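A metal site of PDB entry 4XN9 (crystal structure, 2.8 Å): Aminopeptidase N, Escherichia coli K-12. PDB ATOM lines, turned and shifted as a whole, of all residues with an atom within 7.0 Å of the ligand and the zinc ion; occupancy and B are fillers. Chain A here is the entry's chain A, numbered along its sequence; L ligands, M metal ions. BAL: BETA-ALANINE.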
ATOM      1  N   GLN A 115      16.123  16.009   8.678  1.00  0.00           N
ATOM      2  CA  GLN A 115      17.274  15.163   8.399  1.00  0.00           C
ATOM      3  C   GLN A 115      18.539  15.987   8.531  1.00  0.00           C
ATOM      4  O   GLN A 115      18.720  16.961   7.799  1.00  0.00           O
ATOM      5  CB  GLN A 115      17.181  14.557   6.999  1.00  0.00           C
ATOM      6  CG  GLN A 115      18.430  13.778   6.605  1.00  0.00           C
ATOM      7  CD  GLN A 115      18.735  12.659   7.555  1.00  0.00           C
ATOM      8  OE1 GLN A 115      17.840  12.112   8.214  1.00  0.00           O
ATOM      9  NE2 GLN A 115      19.996  12.288   7.636  1.00  0.00           N
ATOM     10  N   GLU A 117      21.978  14.434   9.073  1.00  0.00           N
ATOM     11  CA  GLU A 117      23.246  13.790   8.628  1.00  0.00           C
ATOM     12  C   GLU A 117      23.419  14.052   7.154  1.00  0.00           C
ATOM     13  O   GLU A 117      22.504  13.789   6.406  1.00  0.00           O
ATOM     14  CB  GLU A 117      23.316  12.265   8.916  1.00  0.00           C
ATOM     15  CG  GLU A 117      24.766  11.748   8.874  1.00  0.00           C
ATOM     16  CD  GLU A 117      24.954  10.264   9.165  1.00  0.00           C
ATOM     17  OE1 GLU A 117      24.007   9.565   9.613  1.00  0.00           O
ATOM     18  OE2 GLU A 117      26.093   9.794   8.977  1.00  0.00           O
ATOM     19  N   TYR A 181      24.267  16.028  14.215  1.00  0.00           N
ATOM     20  CA  TYR A 181      23.679  15.173  13.123  1.00  0.00           C
ATOM     21  C   TYR A 181      22.590  14.195  13.578  1.00  0.00           C
ATOM     22  O   TYR A 181      21.749  13.719  12.793  1.00  0.00           O
ATOM     23  CB  TYR A 181      24.762  14.405  12.316  1.00  0.00           C
ATOM     24  CG  TYR A 181      25.315  13.133  12.921  1.00  0.00           C
ATOM     25  CD1 TYR A 181      24.761  11.905  12.653  1.00  0.00           C
ATOM     26  CD2 TYR A 181      26.461  13.157  13.690  1.00  0.00           C
ATOM     27  CE1 TYR A 181      25.306  10.737  13.178  1.00  0.00           C
ATOM     28  CE2 TYR A 181      27.011  11.982  14.195  1.00  0.00           C
ATOM     29  CZ  TYR A 181      26.432  10.780  13.931  1.00  0.00           C
ATOM     30  OH  TYR A 181      26.995   9.649  14.440  1.00  0.00           O
ATOM     31  N   MET A 256      17.600   9.338   2.661  1.00  0.00           N
ATOM     32  CA  MET A 256      18.234   8.050   3.036  1.00  0.00           C
ATOM     33  C   MET A 256      17.153   6.941   3.097  1.00  0.00           C
ATOM     34  O   MET A 256      15.978   7.106   2.624  1.00  0.00           O
ATOM     35  CB  MET A 256      18.963   8.162   4.362  1.00  0.00           C
ATOM     36  CG  MET A 256      19.697   9.476   4.567  1.00  0.00           C
ATOM     37  SD  MET A 256      21.479   9.223   4.550  1.00  0.00           S
ATOM     38  CE  MET A 256      22.096  10.886   4.177  1.00  0.00           C
ATOM     39  N   GLY A 257      17.537   5.803   3.648  1.00  0.00           N
ATOM     40  CA  GLY A 257      16.536   4.746   3.872  1.00  0.00           C
ATOM     41  C   GLY A 257      15.890   5.007   5.192  1.00  0.00           C
ATOM     42  O   GLY A 257      14.703   5.048   5.296  1.00  0.00           O
ATOM     43  N   ALA A 258      16.745   5.238   6.180  1.00  0.00           N
ATOM     44  CA  ALA A 258      16.381   5.451   7.560  1.00  0.00           C
ATOM     45  C   ALA A 258      17.579   6.093   8.271  1.00  0.00           C
ATOM     46  O   ALA A 258      18.679   6.152   7.729  1.00  0.00           O
ATOM     47  CB  ALA A 258      15.996   4.142   8.201  1.00  0.00           C
ATOM     48  N   MET A 259      17.364   6.574   9.488  1.00  0.00           N
ATOM     49  CA  MET A 259      18.319   7.436  10.136  1.00  0.00           C
ATOM     50  C   MET A 259      18.275   7.230  11.640  1.00  0.00           C
ATOM     51  O   MET A 259      17.225   7.375  12.254  1.00  0.00           O
ATOM     52  CB  MET A 259      17.978   8.901   9.811  1.00  0.00           C
ATOM     53  CG  MET A 259      18.898   9.950  10.443  1.00  0.00           C
ATOM     54  SD  MET A 259      20.642   9.626  10.081  1.00  0.00           S
ATOM     55  CE  MET A 259      21.483  10.108  11.575  1.00  0.00           C
ATOM     56  N   GLU A 260      19.448   6.973  12.219  1.00  0.00           N
ATOM     57  CA  GLU A 260      19.604   6.582  13.611  1.00  0.00           C
ATOM     58  C   GLU A 260      19.515   7.689  14.638  1.00  0.00           C
ATOM     59  O   GLU A 260      20.209   7.603  15.650  1.00  0.00           O
ATOM     60  CB  GLU A 260      20.943   5.845  13.787  1.00  0.00           C
ATOM     61  CG  GLU A 260      22.239   6.661  13.687  1.00  0.00           C
ATOM     62  CD  GLU A 260      22.791   6.822  12.275  1.00  0.00           C
ATOM     63  OE1 GLU A 260      22.061   6.596  11.277  1.00  0.00           O
ATOM     64  OE2 GLU A 260      23.975   7.202  12.139  1.00  0.00           O
ATOM     65  N   VAL A 290      17.055  -3.142   7.882  1.00  0.00           N
ATOM     66  CA  VAL A 290      17.137  -1.708   8.140  1.00  0.00           C
ATOM     67  C   VAL A 290      16.727  -1.241   9.562  1.00  0.00           C
ATOM     68  O   VAL A 290      17.382  -0.383  10.118  1.00  0.00           O
ATOM     69  CB  VAL A 290      16.336  -0.934   7.065  1.00  0.00           C
ATOM     70  CG1 VAL A 290      16.174   0.571   7.384  1.00  0.00           C
ATOM     71  CG2 VAL A 290      16.971  -1.172   5.700  1.00  0.00           C
ATOM     72  N   HIS A 293      19.554  -2.182  11.669  1.00  0.00           N
ATOM     73  CA  HIS A 293      20.685  -1.337  11.361  1.00  0.00           C
ATOM     74  C   HIS A 293      20.572  -0.046  12.181  1.00  0.00           C
ATOM     75  O   HIS A 293      21.528   0.342  12.858  1.00  0.00           O
ATOM     76  CB  HIS A 293      20.716  -1.063   9.851  1.00  0.00           C
ATOM     77  CG  HIS A 293      21.855  -0.216   9.408  1.00  0.00           C
ATOM     78  ND1 HIS A 293      23.068  -0.736   9.015  1.00  0.00           N
ATOM     79  CD2 HIS A 293      21.970   1.132   9.284  1.00  0.00           C
ATOM     80  CE1 HIS A 293      23.894   0.251   8.703  1.00  0.00           C
ATOM     81  NE2 HIS A 293      23.257   1.390   8.871  1.00  0.00           N
ATOM     82  N   GLU A 294      19.436   0.623  12.141  1.00  0.00           N
ATOM     83  CA  GLU A 294      19.319   1.861  12.895  1.00  0.00           C
ATOM     84  C   GLU A 294      19.398   1.576  14.382  1.00  0.00           C
ATOM     85  O   GLU A 294      19.983   2.355  15.132  1.00  0.00           O
ATOM     86  CB  GLU A 294      18.024   2.566  12.582  1.00  0.00           C
ATOM     87  CG  GLU A 294      17.767   2.800  11.097  1.00  0.00           C
ATOM     88  CD  GLU A 294      18.942   3.406  10.298  1.00  0.00           C
ATOM     89  OE1 GLU A 294      19.800   4.136  10.851  1.00  0.00           O
ATOM     90  OE2 GLU A 294      19.021   3.155   9.099  1.00  0.00           O
ATOM     91  N   HIS A 297      23.058   1.093  15.465  1.00  0.00           N
ATOM     92  CA  HIS A 297      23.684   2.412  15.530  1.00  0.00           C
ATOM     93  C   HIS A 297      23.616   3.075  16.918  1.00  0.00           C
ATOM     94  O   HIS A 297      24.436   3.962  17.231  1.00  0.00           O
ATOM     95  CB  HIS A 297      23.037   3.373  14.519  1.00  0.00           C
ATOM     96  CG  HIS A 297      23.742   3.458  13.190  1.00  0.00           C
ATOM     97  ND1 HIS A 297      25.115   3.516  13.080  1.00  0.00           N
ATOM     98  CD2 HIS A 297      23.261   3.498  11.929  1.00  0.00           C
ATOM     99  CE1 HIS A 297      25.445   3.577  11.813  1.00  0.00           C
ATOM    100  NE2 HIS A 297      24.339   3.570  11.094  1.00  0.00           N
ATOM    101  N   THR A 300      26.983   1.747  17.986  1.00  0.00           N
ATOM    102  CA  THR A 300      28.032   1.939  16.964  1.00  0.00           C
ATOM    103  C   THR A 300      27.612   3.102  16.097  1.00  0.00           C
ATOM    104  O   THR A 300      27.071   2.926  14.984  1.00  0.00           O
ATOM    105  CB  THR A 300      28.282   0.669  16.162  1.00  0.00           C
ATOM    106  OG1 THR A 300      27.056   0.185  15.637  1.00  0.00           O
ATOM    107  CG2 THR A 300      28.898  -0.419  17.068  1.00  0.00           C
ATOM    108  N   TRP A 309      33.914  13.479   9.475  1.00  0.00           N
ATOM    109  CA  TRP A 309      33.156  12.681   8.534  1.00  0.00           C
ATOM    110  C   TRP A 309      33.997  11.729   7.679  1.00  0.00           C
ATOM    111  O   TRP A 309      33.496  10.815   7.036  1.00  0.00           O
ATOM    112  CB  TRP A 309      32.280  13.576   7.665  1.00  0.00           C
ATOM    113  CG  TRP A 309      31.145  14.102   8.445  1.00  0.00           C
ATOM    114  CD1 TRP A 309      30.866  15.398   8.704  1.00  0.00           C
ATOM    115  CD2 TRP A 309      30.110  13.327   9.086  1.00  0.00           C
ATOM    116  NE1 TRP A 309      29.723  15.485   9.474  1.00  0.00           N
ATOM    117  CE2 TRP A 309      29.258  14.229   9.724  1.00  0.00           C
ATOM    118  CE3 TRP A 309      29.859  11.957   9.192  1.00  0.00           C
ATOM    119  CZ2 TRP A 309      28.137  13.806  10.462  1.00  0.00           C
ATOM    120  CZ3 TRP A 309      28.743  11.528   9.924  1.00  0.00           C
ATOM    121  CH2 TRP A 309      27.890  12.459  10.552  1.00  0.00           C
ATOM    122  N   LEU A 312      33.448   8.092   8.608  1.00  0.00           N
ATOM    123  CA  LEU A 312      32.103   7.553   8.464  1.00  0.00           C
ATOM    124  C   LEU A 312      32.035   6.020   8.612  1.00  0.00           C
ATOM    125  O   LEU A 312      31.183   5.502   9.313  1.00  0.00           O
ATOM    126  CB  LEU A 312      31.506   7.940   7.108  1.00  0.00           C
ATOM    127  CG  LEU A 312      30.068   7.533   6.914  1.00  0.00           C
ATOM    128  CD1 LEU A 312      29.158   8.086   8.015  1.00  0.00           C
ATOM    129  CD2 LEU A 312      29.607   8.067   5.596  1.00  0.00           C
ATOM    130  N   LYS A 315      31.489   3.913  11.889  1.00  0.00           N
ATOM    131  CA  LYS A 315      30.127   3.532  12.265  1.00  0.00           C
ATOM    132  C   LYS A 315      29.312   2.759  11.177  1.00  0.00           C
ATOM    133  O   LYS A 315      28.477   1.906  11.507  1.00  0.00           O
ATOM    134  CB  LYS A 315      29.369   4.757  12.741  1.00  0.00           C
ATOM    135  CG  LYS A 315      29.040   5.798  11.696  1.00  0.00           C
ATOM    136  CD  LYS A 315      28.172   6.870  12.348  1.00  0.00           C
ATOM    137  CE  LYS A 315      27.746   8.067  11.478  1.00  0.00           C
ATOM    138  NZ  LYS A 315      26.514   7.832  10.706  1.00  0.00           N
ATOM    139  N   GLU A 316      29.530   3.039   9.896  1.00  0.00           N
ATOM    140  CA  GLU A 316      28.737   2.398   8.856  1.00  0.00           C
ATOM    141  C   GLU A 316      29.211   0.980   8.537  1.00  0.00           C
ATOM    142  O   GLU A 316      28.430   0.034   8.401  1.00  0.00           O
ATOM    143  CB  GLU A 316      28.720   3.242   7.585  1.00  0.00           C
ATOM    144  CG  GLU A 316      28.035   4.568   7.772  1.00  0.00           C
ATOM    145  CD  GLU A 316      26.670   4.378   8.389  1.00  0.00           C
ATOM    146  OE1 GLU A 316      26.149   3.263   8.271  1.00  0.00           O
ATOM    147  OE2 GLU A 316      26.137   5.332   9.002  1.00  0.00           O
ATOM    148  N   GLY A 317      30.496   0.802   8.413  1.00  0.00           N
ATOM    149  CA  GLY A 317      30.991  -0.537   8.139  1.00  0.00           C
ATOM    150  C   GLY A 317      30.652  -1.472   9.265  1.00  0.00           C
ATOM    151  O   GLY A 317      30.190  -2.591   9.029  1.00  0.00           O
ATOM    152  N   THR A 319      28.315  -1.016  11.598  1.00  0.00           N
ATOM    153  CA  THR A 319      26.831  -1.174  11.746  1.00  0.00           C
ATOM    154  C   THR A 319      26.201  -2.017  10.608  1.00  0.00           C
ATOM    155  O   THR A 319      25.250  -2.788  10.834  1.00  0.00           O
ATOM    156  CB  THR A 319      26.104   0.179  11.922  1.00  0.00           C
ATOM    157  OG1 THR A 319      26.588   0.817  13.111  1.00  0.00           O
ATOM    158  CG2 THR A 319      24.614  -0.029  12.045  1.00  0.00           C
ATOM    159  N   VAL A 320      26.739  -1.906   9.397  1.00  0.00           N
ATOM    160  CA  VAL A 320      26.430  -2.878   8.341  1.00  0.00           C
ATOM    161  C   VAL A 320      26.862  -4.288   8.758  1.00  0.00           C
ATOM    162  O   VAL A 320      26.092  -5.232   8.630  1.00  0.00           O
ATOM    163  CB  VAL A 320      27.064  -2.501   7.001  1.00  0.00           C
ATOM    164  CG1 VAL A 320      26.977  -3.644   5.996  1.00  0.00           C
ATOM    165  CG2 VAL A 320      26.404  -1.236   6.406  1.00  0.00           C
ATOM    166  N   ASP A 323      24.285  -5.385  11.097  1.00  0.00           N
ATOM    167  CA  ASP A 323      23.015  -5.814  10.487  1.00  0.00           C
ATOM    168  C   ASP A 323      23.093  -7.169   9.691  1.00  0.00           C
ATOM    169  O   ASP A 323      22.087  -7.908   9.642  1.00  0.00           O
ATOM    170  CB  ASP A 323      22.324  -4.664   9.715  1.00  0.00           C
ATOM    171  CG  ASP A 323      22.722  -4.535   8.262  1.00  0.00           C
ATOM    172  OD1 ASP A 323      22.735  -5.573   7.517  1.00  0.00           O
ATOM    173  OD2 ASP A 323      22.973  -3.370   7.831  1.00  0.00           O
ATOM    174  N   TYR A 372      28.149   8.392   1.194  1.00  0.00           N
ATOM    175  CA  TYR A 372      27.281   7.342   1.771  1.00  0.00           C
ATOM    176  C   TYR A 372      27.202   6.272   0.712  1.00  0.00           C
ATOM    177  O   TYR A 372      26.269   6.221  -0.074  1.00  0.00           O
ATOM    178  CB  TYR A 372      25.889   7.926   2.194  1.00  0.00           C
ATOM    179  CG  TYR A 372      26.095   8.778   3.389  1.00  0.00           C
ATOM    180  CD1 TYR A 372      26.634  10.064   3.268  1.00  0.00           C
ATOM    181  CD2 TYR A 372      25.984   8.240   4.666  1.00  0.00           C
ATOM    182  CE1 TYR A 372      26.949  10.822   4.369  1.00  0.00           C
ATOM    183  CE2 TYR A 372      26.292   8.991   5.782  1.00  0.00           C
ATOM    184  CZ  TYR A 372      26.756  10.279   5.629  1.00  0.00           C
ATOM    185  OH  TYR A 372      27.067  11.013   6.731  1.00  0.00           O
ATOM    186  N   TYR A 377      29.988   1.701   3.189  1.00  0.00           N
ATOM    187  CA  TYR A 377      29.068   0.774   3.868  1.00  0.00           C
ATOM    188  C   TYR A 377      29.438  -0.692   3.690  1.00  0.00           C
ATOM    189  O   TYR A 377      29.784  -1.376   4.681  1.00  0.00           O
ATOM    190  CB  TYR A 377      27.651   0.950   3.355  1.00  0.00           C
ATOM    191  CG  TYR A 377      26.941   2.117   3.951  1.00  0.00           C
ATOM    192  CD1 TYR A 377      27.400   3.368   3.793  1.00  0.00           C
ATOM    193  CD2 TYR A 377      25.801   1.922   4.713  1.00  0.00           C
ATOM    194  CE1 TYR A 377      26.731   4.438   4.334  1.00  0.00           C
ATOM    195  CE2 TYR A 377      25.131   2.966   5.306  1.00  0.00           C
ATOM    196  CZ  TYR A 377      25.578   4.241   5.104  1.00  0.00           C
ATOM    197  OH  TYR A 377      24.900   5.307   5.687  1.00  0.00           O
HETATM  198  N   BAL L   1      23.902   7.108   8.863  1.00  0.00           N
HETATM  199  CB  BAL L   1      22.541   7.301   8.429  1.00  0.00           C
HETATM  200  CA  BAL L   1      21.937   6.231   7.551  1.00  0.00           C
HETATM  201  C   BAL L   1      22.359   4.902   8.047  1.00  0.00           C
HETATM  202  O   BAL L   1      21.540   4.208   8.614  1.00  0.00           O
HETATM  203  OXT BAL L   1      23.537   4.575   7.864  1.00  0.00           O
HETATM  204 ZN    ZN M   1      24.125   3.299   9.046  1.00  0.00          ZN
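Residues that only touch the ligand: Ala 258 (3.3 Å) and Met 259 (3.4 Å).
Hydrophobic or aromatic side chains that line the ligand: Met 259, His 293, His 297 and Tyr 377.
An oxygen (OXT) of the ligand is bound to the zinc ion.
A ring nitrogen (NE2) of His 297 is bound to the zinc ion, at 2.1 Å.
A ring nitrogen (NE2) of His 293 binds the zinc ion (2.1 Å).
The zinc ion is bound by OE1 of Glu 316.
Slightly farther from the zinc ion lies O of the ligand (2.8 Å).
OE1 of Glu 260 is in salt-bridge range of N of the ligand, 3.1 Å away.
The side-chain hydroxyl of Tyr 377 lies close to an oxygen (OXT) of the ligand (2.7 Å).
An oxygen (O) of the ligand sits close to the side-chain carboxylate of Glu 294.
OE1 of Glu 117 is in salt-bridge range of N of the ligand (2.6 Å).
NZ of Lys 315 lies close to N of the ligand (3.3 Å).
N of Glu 260 sits at hydrogen-bond distance from OE1 of Glu 294, at 3.2 Å.
The backbone carbonyl oxygen of Lys 315 lies within hydrogen-bond range of the side-chain hydroxyl of Thr 319 (2.7 Å).
The side-chain carboxylate of Glu 260 lies within salt-bridge range of the side-chain amino group of Lys 315, 3.0 Å away.
The side-chain amide nitrogen of Gln 115 sits at hydrogen-bond distance from the side-chain sulfur of Met 259.
OE2 of Glu 316 lies within salt-bridge range of NZ of Lys 315.
The side-chain hydroxyl (OG1) of Thr 319 lies within hydrogen-bond range of a ring nitrogen (ND1) of His 297, 3.1 Å away.
ND1 of His 297 sits at hydrogen-bond distance from O of Thr 300 (2.8 Å).
The backbone carbonyl oxygen (O) of Glu 117 lies within hydrogen-bond range of the side-chain amide nitrogen (NE2) of Gln 115, 3.2 Å away.
Residues that only touch the zinc ion: Tyr 377 (3.9 Å).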
